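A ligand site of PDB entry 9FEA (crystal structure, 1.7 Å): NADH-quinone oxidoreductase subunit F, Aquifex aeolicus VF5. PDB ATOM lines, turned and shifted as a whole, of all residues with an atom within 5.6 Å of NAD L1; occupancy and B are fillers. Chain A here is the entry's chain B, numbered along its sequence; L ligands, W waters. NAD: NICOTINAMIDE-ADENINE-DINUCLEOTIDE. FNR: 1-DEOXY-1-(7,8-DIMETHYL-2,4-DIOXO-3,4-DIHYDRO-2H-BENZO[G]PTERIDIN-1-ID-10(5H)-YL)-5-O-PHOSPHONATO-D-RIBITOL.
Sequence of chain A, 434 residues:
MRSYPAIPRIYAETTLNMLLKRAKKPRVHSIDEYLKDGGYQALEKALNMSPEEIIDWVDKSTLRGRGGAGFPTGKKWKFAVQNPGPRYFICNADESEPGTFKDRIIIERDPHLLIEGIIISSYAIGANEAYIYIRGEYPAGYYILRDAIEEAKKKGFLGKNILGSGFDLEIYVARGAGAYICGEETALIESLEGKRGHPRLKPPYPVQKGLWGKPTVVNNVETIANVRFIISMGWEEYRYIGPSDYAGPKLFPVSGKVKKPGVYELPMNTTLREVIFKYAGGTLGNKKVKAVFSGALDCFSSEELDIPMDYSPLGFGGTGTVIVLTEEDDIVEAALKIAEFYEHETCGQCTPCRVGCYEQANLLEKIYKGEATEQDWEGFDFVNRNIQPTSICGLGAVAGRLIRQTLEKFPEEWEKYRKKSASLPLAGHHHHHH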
ATOM      1  N   GLY A  67      10.562  -8.957  -7.412  1.00  0.00           N
ATOM      2  CA  GLY A  67      11.226  -9.873  -6.494  1.00  0.00           C
ATOM      3  C   GLY A  67      12.553 -10.386  -7.042  1.00  0.00           C
ATOM      4  O   GLY A  67      13.218 -11.169  -6.351  1.00  0.00           O
ATOM      5  N   GLY A  68      12.937  -9.952  -8.259  1.00  0.00           N
ATOM      6  CA  GLY A  68      14.263 -10.239  -8.781  1.00  0.00           C
ATOM      7  C   GLY A  68      14.239 -10.834 -10.190  1.00  0.00           C
ATOM      8  O   GLY A  68      15.218 -10.712 -10.931  1.00  0.00           O
ATOM      9  N   ALA A  69      13.151 -11.505 -10.567  1.00  0.00           N
ATOM     10  CA  ALA A  69      13.150 -12.236 -11.839  1.00  0.00           C
ATOM     11  C   ALA A  69      12.473 -11.439 -12.952  1.00  0.00           C
ATOM     12  O   ALA A  69      12.630 -11.814 -14.114  1.00  0.00           O
ATOM     13  CB  ALA A  69      12.475 -13.566 -11.698  1.00  0.00           C
ATOM     14  N   PHE A  71       9.308 -11.270 -14.003  1.00  0.00           N
ATOM     15  CA  PHE A  71       8.276 -11.925 -14.798  1.00  0.00           C
ATOM     16  C   PHE A  71       7.043 -11.031 -14.937  1.00  0.00           C
ATOM     17  O   PHE A  71       6.612 -10.403 -13.977  1.00  0.00           O
ATOM     18  CB  PHE A  71       7.846 -13.276 -14.240  1.00  0.00           C
ATOM     19  CG  PHE A  71       7.096 -14.124 -15.250  1.00  0.00           C
ATOM     20  CD1 PHE A  71       7.777 -14.950 -16.136  1.00  0.00           C
ATOM     21  CD2 PHE A  71       5.708 -14.140 -15.280  1.00  0.00           C
ATOM     22  CE1 PHE A  71       7.090 -15.747 -17.056  1.00  0.00           C
ATOM     23  CE2 PHE A  71       5.021 -14.938 -16.190  1.00  0.00           C
ATOM     24  CZ  PHE A  71       5.723 -15.741 -17.072  1.00  0.00           C
ATOM     25  N   LYS A  76       1.456 -13.715 -15.464  1.00  0.00           N
ATOM     26  CA  LYS A  76       1.424 -14.678 -14.374  1.00  0.00           C
ATOM     27  C   LYS A  76      -0.020 -14.912 -13.918  1.00  0.00           C
ATOM     28  O   LYS A  76      -0.473 -16.060 -13.783  1.00  0.00           O
ATOM     29  CB  LYS A  76       2.347 -14.213 -13.245  1.00  0.00           C
ATOM     30  CG  LYS A  76       2.513 -15.250 -12.130  1.00  0.00           C
ATOM     31  CD  LYS A  76       3.202 -14.740 -10.890  1.00  0.00           C
ATOM     32  CE  LYS A  76       4.608 -14.313 -11.155  1.00  0.00           C
ATOM     33  NZ  LYS A  76       5.291 -14.027  -9.890  1.00  0.00           N
ATOM     34  N   PHE A  79      -2.076 -16.923 -16.352  1.00  0.00           N
ATOM     35  CA  PHE A  79      -1.760 -18.347 -16.289  1.00  0.00           C
ATOM     36  C   PHE A  79      -2.529 -19.024 -15.154  1.00  0.00           C
ATOM     37  O   PHE A  79      -3.047 -20.127 -15.341  1.00  0.00           O
ATOM     38  CB  PHE A  79      -0.248 -18.554 -16.175  1.00  0.00           C
ATOM     39  CG  PHE A  79       0.542 -18.381 -17.467  1.00  0.00           C
ATOM     40  CD1 PHE A  79       0.023 -18.785 -18.695  1.00  0.00           C
ATOM     41  CD2 PHE A  79       1.806 -17.801 -17.452  1.00  0.00           C
ATOM     42  CE1 PHE A  79       0.761 -18.627 -19.870  1.00  0.00           C
ATOM     43  CE2 PHE A  79       2.544 -17.666 -18.620  1.00  0.00           C
ATOM     44  CZ  PHE A  79       2.013 -18.056 -19.817  1.00  0.00           C
ATOM     45  N   GLU A  97      17.732 -10.822   0.994  1.00  0.00           N
ATOM     46  CA  GLU A  97      18.979 -10.712   0.269  1.00  0.00           C
ATOM     47  C   GLU A  97      19.817  -9.561   0.805  1.00  0.00           C
ATOM     48  O   GLU A  97      19.267  -8.460   1.004  1.00  0.00           O
ATOM     49  CB  GLU A  97      18.748 -10.475  -1.221  1.00  0.00           C
ATOM     50  CG  GLU A  97      20.036 -10.694  -2.010  1.00  0.00           C
ATOM     51  CD  GLU A  97      19.912 -10.649  -3.505  1.00  0.00           C
ATOM     52  OE1 GLU A  97      18.772 -10.547  -4.021  1.00  0.00           O
ATOM     53  OE2 GLU A  97      20.960 -10.712  -4.171  1.00  0.00           O
ATOM     54  N   GLU A 184      12.327 -18.084  -1.879  1.00  0.00           N
ATOM     55  CA  GLU A 184      12.081 -18.769  -3.141  1.00  0.00           C
ATOM     56  C   GLU A 184      10.635 -19.261  -3.087  1.00  0.00           C
ATOM     57  O   GLU A 184      10.243 -19.899  -2.114  1.00  0.00           O
ATOM     58  CB  GLU A 184      13.058 -19.921  -3.308  1.00  0.00           C
ATOM     59  CG  GLU A 184      13.078 -20.514  -4.714  1.00  0.00           C
ATOM     60  CD  GLU A 184      11.945 -21.468  -5.045  1.00  0.00           C
ATOM     61  OE1 GLU A 184      11.433 -22.067  -4.106  1.00  0.00           O
ATOM     62  OE2 GLU A 184      11.534 -21.564  -6.201  1.00  0.00           O
ATOM     63  N   GLU A 185       9.855 -18.964  -4.122  1.00  0.00           N
ATOM     64  CA  GLU A 185       8.404 -19.106  -4.018  1.00  0.00           C
ATOM     65  C   GLU A 185       7.962 -20.521  -3.620  1.00  0.00           C
ATOM     66  O   GLU A 185       6.984 -20.641  -2.900  1.00  0.00           O
ATOM     67  CB  GLU A 185       7.706 -18.653  -5.293  1.00  0.00           C
ATOM     68  CG  GLU A 185       8.091 -19.471  -6.509  1.00  0.00           C
ATOM     69  CD  GLU A 185       7.476 -19.014  -7.818  1.00  0.00           C
ATOM     70  OE1 GLU A 185       6.661 -18.060  -7.794  1.00  0.00           O
ATOM     71  OE2 GLU A 185       7.860 -19.606  -8.838  1.00  0.00           O
ATOM     72  N   LYS A 202      10.695 -27.098 -10.575  1.00  0.00           N
ATOM     73  CA  LYS A 202       9.851 -26.234 -11.379  1.00  0.00           C
ATOM     74  C   LYS A 202      10.288 -26.385 -12.830  1.00  0.00           C
ATOM     75  O   LYS A 202      11.487 -26.417 -13.090  1.00  0.00           O
ATOM     76  CB  LYS A 202       9.979 -24.737 -11.092  1.00  0.00           C
ATOM     77  CG  LYS A 202       9.505 -24.243  -9.756  1.00  0.00           C
ATOM     78  CD  LYS A 202       9.294 -22.722  -9.710  1.00  0.00           C
ATOM     79  CE  LYS A 202      10.501 -21.863 -10.011  1.00  0.00           C
ATOM     80  NZ  LYS A 202      10.486 -20.584  -9.274  1.00  0.00           N
ATOM     81  N   TYR A 205       4.984 -24.673 -12.291  1.00  0.00           N
ATOM     82  CA  TYR A 205       5.028 -23.378 -11.639  1.00  0.00           C
ATOM     83  C   TYR A 205       3.872 -23.320 -10.638  1.00  0.00           C
ATOM     84  O   TYR A 205       2.901 -24.048 -10.782  1.00  0.00           O
ATOM     85  CB  TYR A 205       4.985 -22.233 -12.653  1.00  0.00           C
ATOM     86  CG  TYR A 205       6.226 -22.162 -13.524  1.00  0.00           C
ATOM     87  CD1 TYR A 205       7.391 -21.569 -13.050  1.00  0.00           C
ATOM     88  CD2 TYR A 205       6.241 -22.734 -14.797  1.00  0.00           C
ATOM     89  CE1 TYR A 205       8.536 -21.512 -13.828  1.00  0.00           C
ATOM     90  CE2 TYR A 205       7.379 -22.680 -15.585  1.00  0.00           C
ATOM     91  CZ  TYR A 205       8.523 -22.054 -15.099  1.00  0.00           C
ATOM     92  OH  TYR A 205       9.647 -22.020 -15.881  1.00  0.00           O
ATOM     93  N   PRO A 206       3.973 -22.471  -9.589  1.00  0.00           N
ATOM     94  CA  PRO A 206       2.896 -22.346  -8.595  1.00  0.00           C
ATOM     95  C   PRO A 206       1.521 -22.071  -9.186  1.00  0.00           C
ATOM     96  O   PRO A 206       0.526 -22.497  -8.632  1.00  0.00           O
ATOM     97  CB  PRO A 206       3.369 -21.218  -7.702  1.00  0.00           C
ATOM     98  CG  PRO A 206       4.881 -21.272  -7.803  1.00  0.00           C
ATOM     99  CD  PRO A 206       5.178 -21.698  -9.223  1.00  0.00           C
ATOM    100  N   VAL A 207       1.481 -21.363 -10.320  1.00  0.00           N
ATOM    101  CA  VAL A 207       0.210 -20.961 -10.921  1.00  0.00           C
ATOM    102  C   VAL A 207      -0.525 -22.209 -11.400  1.00  0.00           C
ATOM    103  O   VAL A 207      -1.725 -22.129 -11.609  1.00  0.00           O
ATOM    104  CB  VAL A 207       0.343 -19.906 -12.034  1.00  0.00           C
ATOM    105  CG1 VAL A 207       0.795 -18.558 -11.481  1.00  0.00           C
ATOM    106  CG2 VAL A 207       1.224 -20.371 -13.169  1.00  0.00           C
ATOM    107  N   VAL A 218       2.267 -16.150  -6.500  1.00  0.00           N
ATOM    108  CA  VAL A 218       3.184 -15.499  -5.592  1.00  0.00           C
ATOM    109  C   VAL A 218       3.672 -14.211  -6.253  1.00  0.00           C
ATOM    110  O   VAL A 218       4.176 -14.246  -7.364  1.00  0.00           O
ATOM    111  CB  VAL A 218       4.385 -16.403  -5.253  1.00  0.00           C
ATOM    112  CG1 VAL A 218       5.285 -15.748  -4.225  1.00  0.00           C
ATOM    113  CG2 VAL A 218       3.932 -17.772  -4.790  1.00  0.00           C
ATOM    114  N   LEU A 297      24.047 -10.854  -6.007  1.00  0.00           N
ATOM    115  CA  LEU A 297      23.910 -11.426  -7.350  1.00  0.00           C
ATOM    116  C   LEU A 297      25.038 -11.043  -8.314  1.00  0.00           C
ATOM    117  O   LEU A 297      25.508 -11.895  -9.055  1.00  0.00           O
ATOM    118  CB  LEU A 297      22.568 -10.985  -7.921  1.00  0.00           C
ATOM    119  CG  LEU A 297      22.226 -11.507  -9.312  1.00  0.00           C
ATOM    120  CD1 LEU A 297      22.137 -13.016  -9.305  1.00  0.00           C
ATOM    121  CD2 LEU A 297      20.919 -10.882  -9.779  1.00  0.00           C
ATOM    122  N   GLY A 318      18.196  -7.180 -11.444  1.00  0.00           N
ATOM    123  CA  GLY A 318      17.987  -7.652 -10.089  1.00  0.00           C
ATOM    124  C   GLY A 318      16.756  -7.025  -9.432  1.00  0.00           C
ATOM    125  O   GLY A 318      15.693  -6.896 -10.040  1.00  0.00           O
ATOM    126  N   GLY A 394      17.227 -21.138  -7.957  1.00  0.00           N
ATOM    127  CA  GLY A 394      18.137 -20.069  -8.364  1.00  0.00           C
ATOM    128  C   GLY A 394      19.325 -19.855  -7.427  1.00  0.00           C
ATOM    129  O   GLY A 394      20.300 -19.254  -7.852  1.00  0.00           O
ATOM    130  N   VAL A 398      23.288 -19.107  -8.794  1.00  0.00           N
ATOM    131  CA  VAL A 398      23.947 -17.804  -8.687  1.00  0.00           C
ATOM    132  C   VAL A 398      24.962 -17.759  -7.548  1.00  0.00           C
ATOM    133  O   VAL A 398      25.632 -16.767  -7.354  1.00  0.00           O
ATOM    134  CB  VAL A 398      22.946 -16.640  -8.560  1.00  0.00           C
ATOM    135  CG1 VAL A 398      21.928 -16.642  -9.674  1.00  0.00           C
ATOM    136  CG2 VAL A 398      22.247 -16.618  -7.201  1.00  0.00           C
HETATM  137  PA  NAD L   1      11.818 -17.519 -12.284  1.00  0.00           P
HETATM  138  O1A NAD L   1      12.424 -16.739 -13.398  1.00  0.00           O
HETATM  139  O2A NAD L   1      11.809 -19.013 -12.341  1.00  0.00           O
HETATM  140  O5B NAD L   1      10.289 -17.057 -12.098  1.00  0.00           O
HETATM  141  C5B NAD L   1       9.896 -15.744 -11.704  1.00  0.00           C
HETATM  142  C4B NAD L   1       8.410 -15.759 -11.417  1.00  0.00           C
HETATM  143  O4B NAD L   1       7.703 -16.003 -12.669  1.00  0.00           O
HETATM  144  C3B NAD L   1       7.936 -16.866 -10.472  1.00  0.00           C
HETATM  145  O3B NAD L   1       6.773 -16.505  -9.740  1.00  0.00           O
HETATM  146  C2B NAD L   1       7.608 -18.009 -11.448  1.00  0.00           C
HETATM  147  O2B NAD L   1       6.683 -18.912 -10.913  1.00  0.00           O
HETATM  148  C1B NAD L   1       7.015 -17.230 -12.609  1.00  0.00           C
HETATM  149  N9A NAD L   1       7.157 -17.902 -13.905  1.00  0.00           N
HETATM  150  C8A NAD L   1       8.282 -17.994 -14.690  1.00  0.00           C
HETATM  151  N7A NAD L   1       8.083 -18.628 -15.813  1.00  0.00           N
HETATM  152  C5A NAD L   1       6.740 -18.993 -15.768  1.00  0.00           C
HETATM  153  C6A NAD L   1       5.932 -19.697 -16.675  1.00  0.00           C
HETATM  154  N6A NAD L   1       6.362 -20.172 -17.840  1.00  0.00           N
HETATM  155  N1A NAD L   1       4.628 -19.867 -16.334  1.00  0.00           N
HETATM  156  C2A NAD L   1       4.201 -19.381 -15.157  1.00  0.00           C
HETATM  157  N3A NAD L   1       4.878 -18.692 -14.240  1.00  0.00           N
HETATM  158  C4A NAD L   1       6.163 -18.543 -14.605  1.00  0.00           C
HETATM  159  O3  NAD L   1      12.594 -17.035 -10.980  1.00  0.00           O
HETATM  160  PN  NAD L   1      12.763 -17.504  -9.449  1.00  0.00           P
HETATM  161  O1N NAD L   1      13.301 -18.904  -9.430  1.00  0.00           O
HETATM  162  O2N NAD L   1      11.459 -17.277  -8.750  1.00  0.00           O
HETATM  163  O5D NAD L   1      13.860 -16.474  -8.890  1.00  0.00           O
HETATM  164  C5D NAD L   1      15.207 -16.458  -9.448  1.00  0.00           C
HETATM  165  C4D NAD L   1      15.451 -15.124 -10.099  1.00  0.00           C
HETATM  166  O4D NAD L   1      14.720 -14.106  -9.377  1.00  0.00           O
HETATM  167  C3D NAD L   1      16.897 -14.601 -10.100  1.00  0.00           C
HETATM  168  O3D NAD L   1      17.068 -13.667 -11.164  1.00  0.00           O
HETATM  169  C2D NAD L   1      17.001 -13.984  -8.693  1.00  0.00           C
HETATM  170  O2D NAD L   1      17.925 -12.913  -8.584  1.00  0.00           O
HETATM  171  C1D NAD L   1      15.592 -13.411  -8.487  1.00  0.00           C
HETATM  172  N1N NAD L   1      15.014 -13.527  -7.125  1.00  0.00           N
HETATM  173  C9A FNR L   2      13.732 -15.507  -4.424  1.00  0.00           C
HETATM  174  N10 FNR L   2      12.633 -14.653  -4.721  1.00  0.00           N
HETATM  175  CAA FNR L   2      12.228 -13.759  -3.760  1.00  0.00           C
HETATM  176  N1  FNR L   2      11.100 -13.025  -4.032  1.00  0.00           N
HETATM  177  C2  FNR L   2      10.582 -12.143  -3.130  1.00  0.00           C
HETATM  178  O2  FNR L   2       9.525 -11.546  -3.362  1.00  0.00           O
HETATM  179  N3  FNR L   2      11.246 -12.011  -1.953  1.00  0.00           N
HETATM  180  C4  FNR L   2      12.368 -12.723  -1.548  1.00  0.00           C
HETATM  181  O4  FNR L   2      12.818 -12.545  -0.430  1.00  0.00           O
HETATM  182  C4A FNR L   2      12.853 -13.627  -2.556  1.00  0.00           C
HETATM  183  N5  FNR L   2      13.909 -14.450  -2.238  1.00  0.00           N
HETATM  184  C5A FNR L   2      14.342 -15.400  -3.163  1.00  0.00           C
HETATM  185  C6  FNR L   2      15.415 -16.237  -2.836  1.00  0.00           C
HETATM  186  C7  FNR L   2      15.865 -17.178  -3.759  1.00  0.00           C
HETATM  187  C7M FNR L   2      17.055 -18.044  -3.407  1.00  0.00           C
HETATM  188  C8  FNR L   2      15.251 -17.277  -5.019  1.00  0.00           C
HETATM  189  C8M FNR L   2      15.755 -18.224  -6.071  1.00  0.00           C
HETATM  190  C9  FNR L   2      14.182 -16.449  -5.348  1.00  0.00           C
HETATM  191  C1' FNR L   2      11.903 -14.770  -5.981  1.00  0.00           C
HETATM  192  C2' FNR L   2      10.639 -15.615  -5.834  1.00  0.00           C
HETATM  193  O2' FNR L   2      10.982 -16.996  -5.997  1.00  0.00           O
HETATM  194  C3' FNR L   2       9.599 -15.199  -6.872  1.00  0.00           C
HETATM  195  O3' FNR L   2      10.152 -15.032  -8.169  1.00  0.00           O
HETATM  196  C4' FNR L   2       8.876 -13.893  -6.570  1.00  0.00           C
HETATM  197  O4' FNR L   2       8.480 -13.815  -5.216  1.00  0.00           O
HETATM  198  C5' FNR L   2       7.725 -13.729  -7.533  1.00  0.00           C
HETATM  199  O5' FNR L   2       7.121 -12.429  -7.325  1.00  0.00           O
HETATM  200  P   FNR L   2       7.274 -11.281  -8.447  1.00  0.00           P
HETATM  201  O1P FNR L   2       6.889 -11.818  -9.802  1.00  0.00           O
HETATM  202  O2P FNR L   2       6.341 -10.175  -7.970  1.00  0.00           O
HETATM  203  O3P FNR L   2       8.726 -10.862  -8.408  1.00  0.00           O
HETATM  204  O   HOH W   1       3.124 -21.722 -17.353  1.00  0.00           O
HETATM  205  O   HOH W   2      10.332 -17.620 -17.653  1.00  0.00           O
HETATM  206  O   HOH W   3      11.769 -20.175 -15.165  1.00  0.00           O
HETATM  207  O   HOH W   4      19.401 -15.273 -11.830  1.00  0.00           O
HETATM  208  O   HOH W   5      17.697 -11.070 -10.631  1.00  0.00           O
HETATM  209  O   HOH W   6      11.233 -15.689 -15.272  1.00  0.00           O
HETATM  210  O   HOH W   7       6.064 -17.633 -20.186  1.00  0.00           O
HETATM  211  O   HOH W   8      14.320 -20.750  -8.180  1.00  0.00           O
HETATM  212  O   HOH W   9       4.070 -18.923 -11.272  1.00  0.00           O
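Water W8 lies within hydrogen-bond range of an oxygen (O1N) of NAD L1 (2.5 Å) and the backbone NH (N) of Gly 394 (2.9 Å). Water W5 bridges the backbone carbonyl oxygen (O) of Gly 68 and an oxygen (O3D) of NAD L1. Water W3 bridges OH of Tyr 205 and O2A of NAD L1.
NZ of Lys 202 lies within salt-bridge range of OE2 of Glu 185. The side-chain amino group (NZ) of Lys 76 is in hydrogen-bond range of the backbone carbonyl oxygen (O) of Val 218, 2.8 Å away. The side-chain carboxylate of Glu 184 lies within salt-bridge range of the side-chain amino group of Lys 202 (3.4 Å).
O2N of NAD L1 sits at hydrogen-bond distance from O3' of FNR L2, 2.7 Å away.
The backbone carbonyl oxygen (O) of Gly 67 lies close to a nitrogen (N1N) of NAD L1 (3.1 Å). Phe 71 touches NAD L1 (CB to O4B, 3.2 Å). Phe 79 touches NAD L1. CD1 of Tyr 205 touches O2B of NAD L1, 3.5 Å away. Pro 206 touches NAD L1. CG2 of Val 207 touches C2A of NAD L1, at 3.7 Å. CD2 of Leu 297 touches O2D of NAD L1, 3.8 Å away. Hydrophobic or aromatic side chains within 4 Å of NAD L1: Ala 69, Phe 71, Phe 79, Tyr 205, Pro 206, Val 207 and Leu 297. The nearest printed residue that does not touch NAD L1 is Val 218 (4.2 Å).
The side-chain carboxylate (OE2) of Glu 185 sits at hydrogen-bond distance from an oxygen (O2B) of NAD L1. NZ of Lys 76 lies within hydrogen-bond range of O3B of NAD L1, 2.9 Å away. An oxygen (O4D) of NAD L1 is in hydrogen-bond range of the backbone NH (N) of Ala 69, 3.3 Å away. The side-chain amino group (NZ) of Lys 202 lies within salt-bridge range of an oxygen (O1N) of NAD L1 (3.3 Å). The backbone carbonyl oxygen (O) of Gly 68 lies within hydrogen-bond range of an oxygen (O3D) of NAD L1 (3.5 Å). O2' of FNR L2 sits at hydrogen-bond distance from N of Glu 185. O1P of FNR L2 lies within salt-bridge range of NZ of Lys 76, 2.7 Å away. N of Gly 67 lies within hydrogen-bond range of O3P of FNR L2 (2.8 Å).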
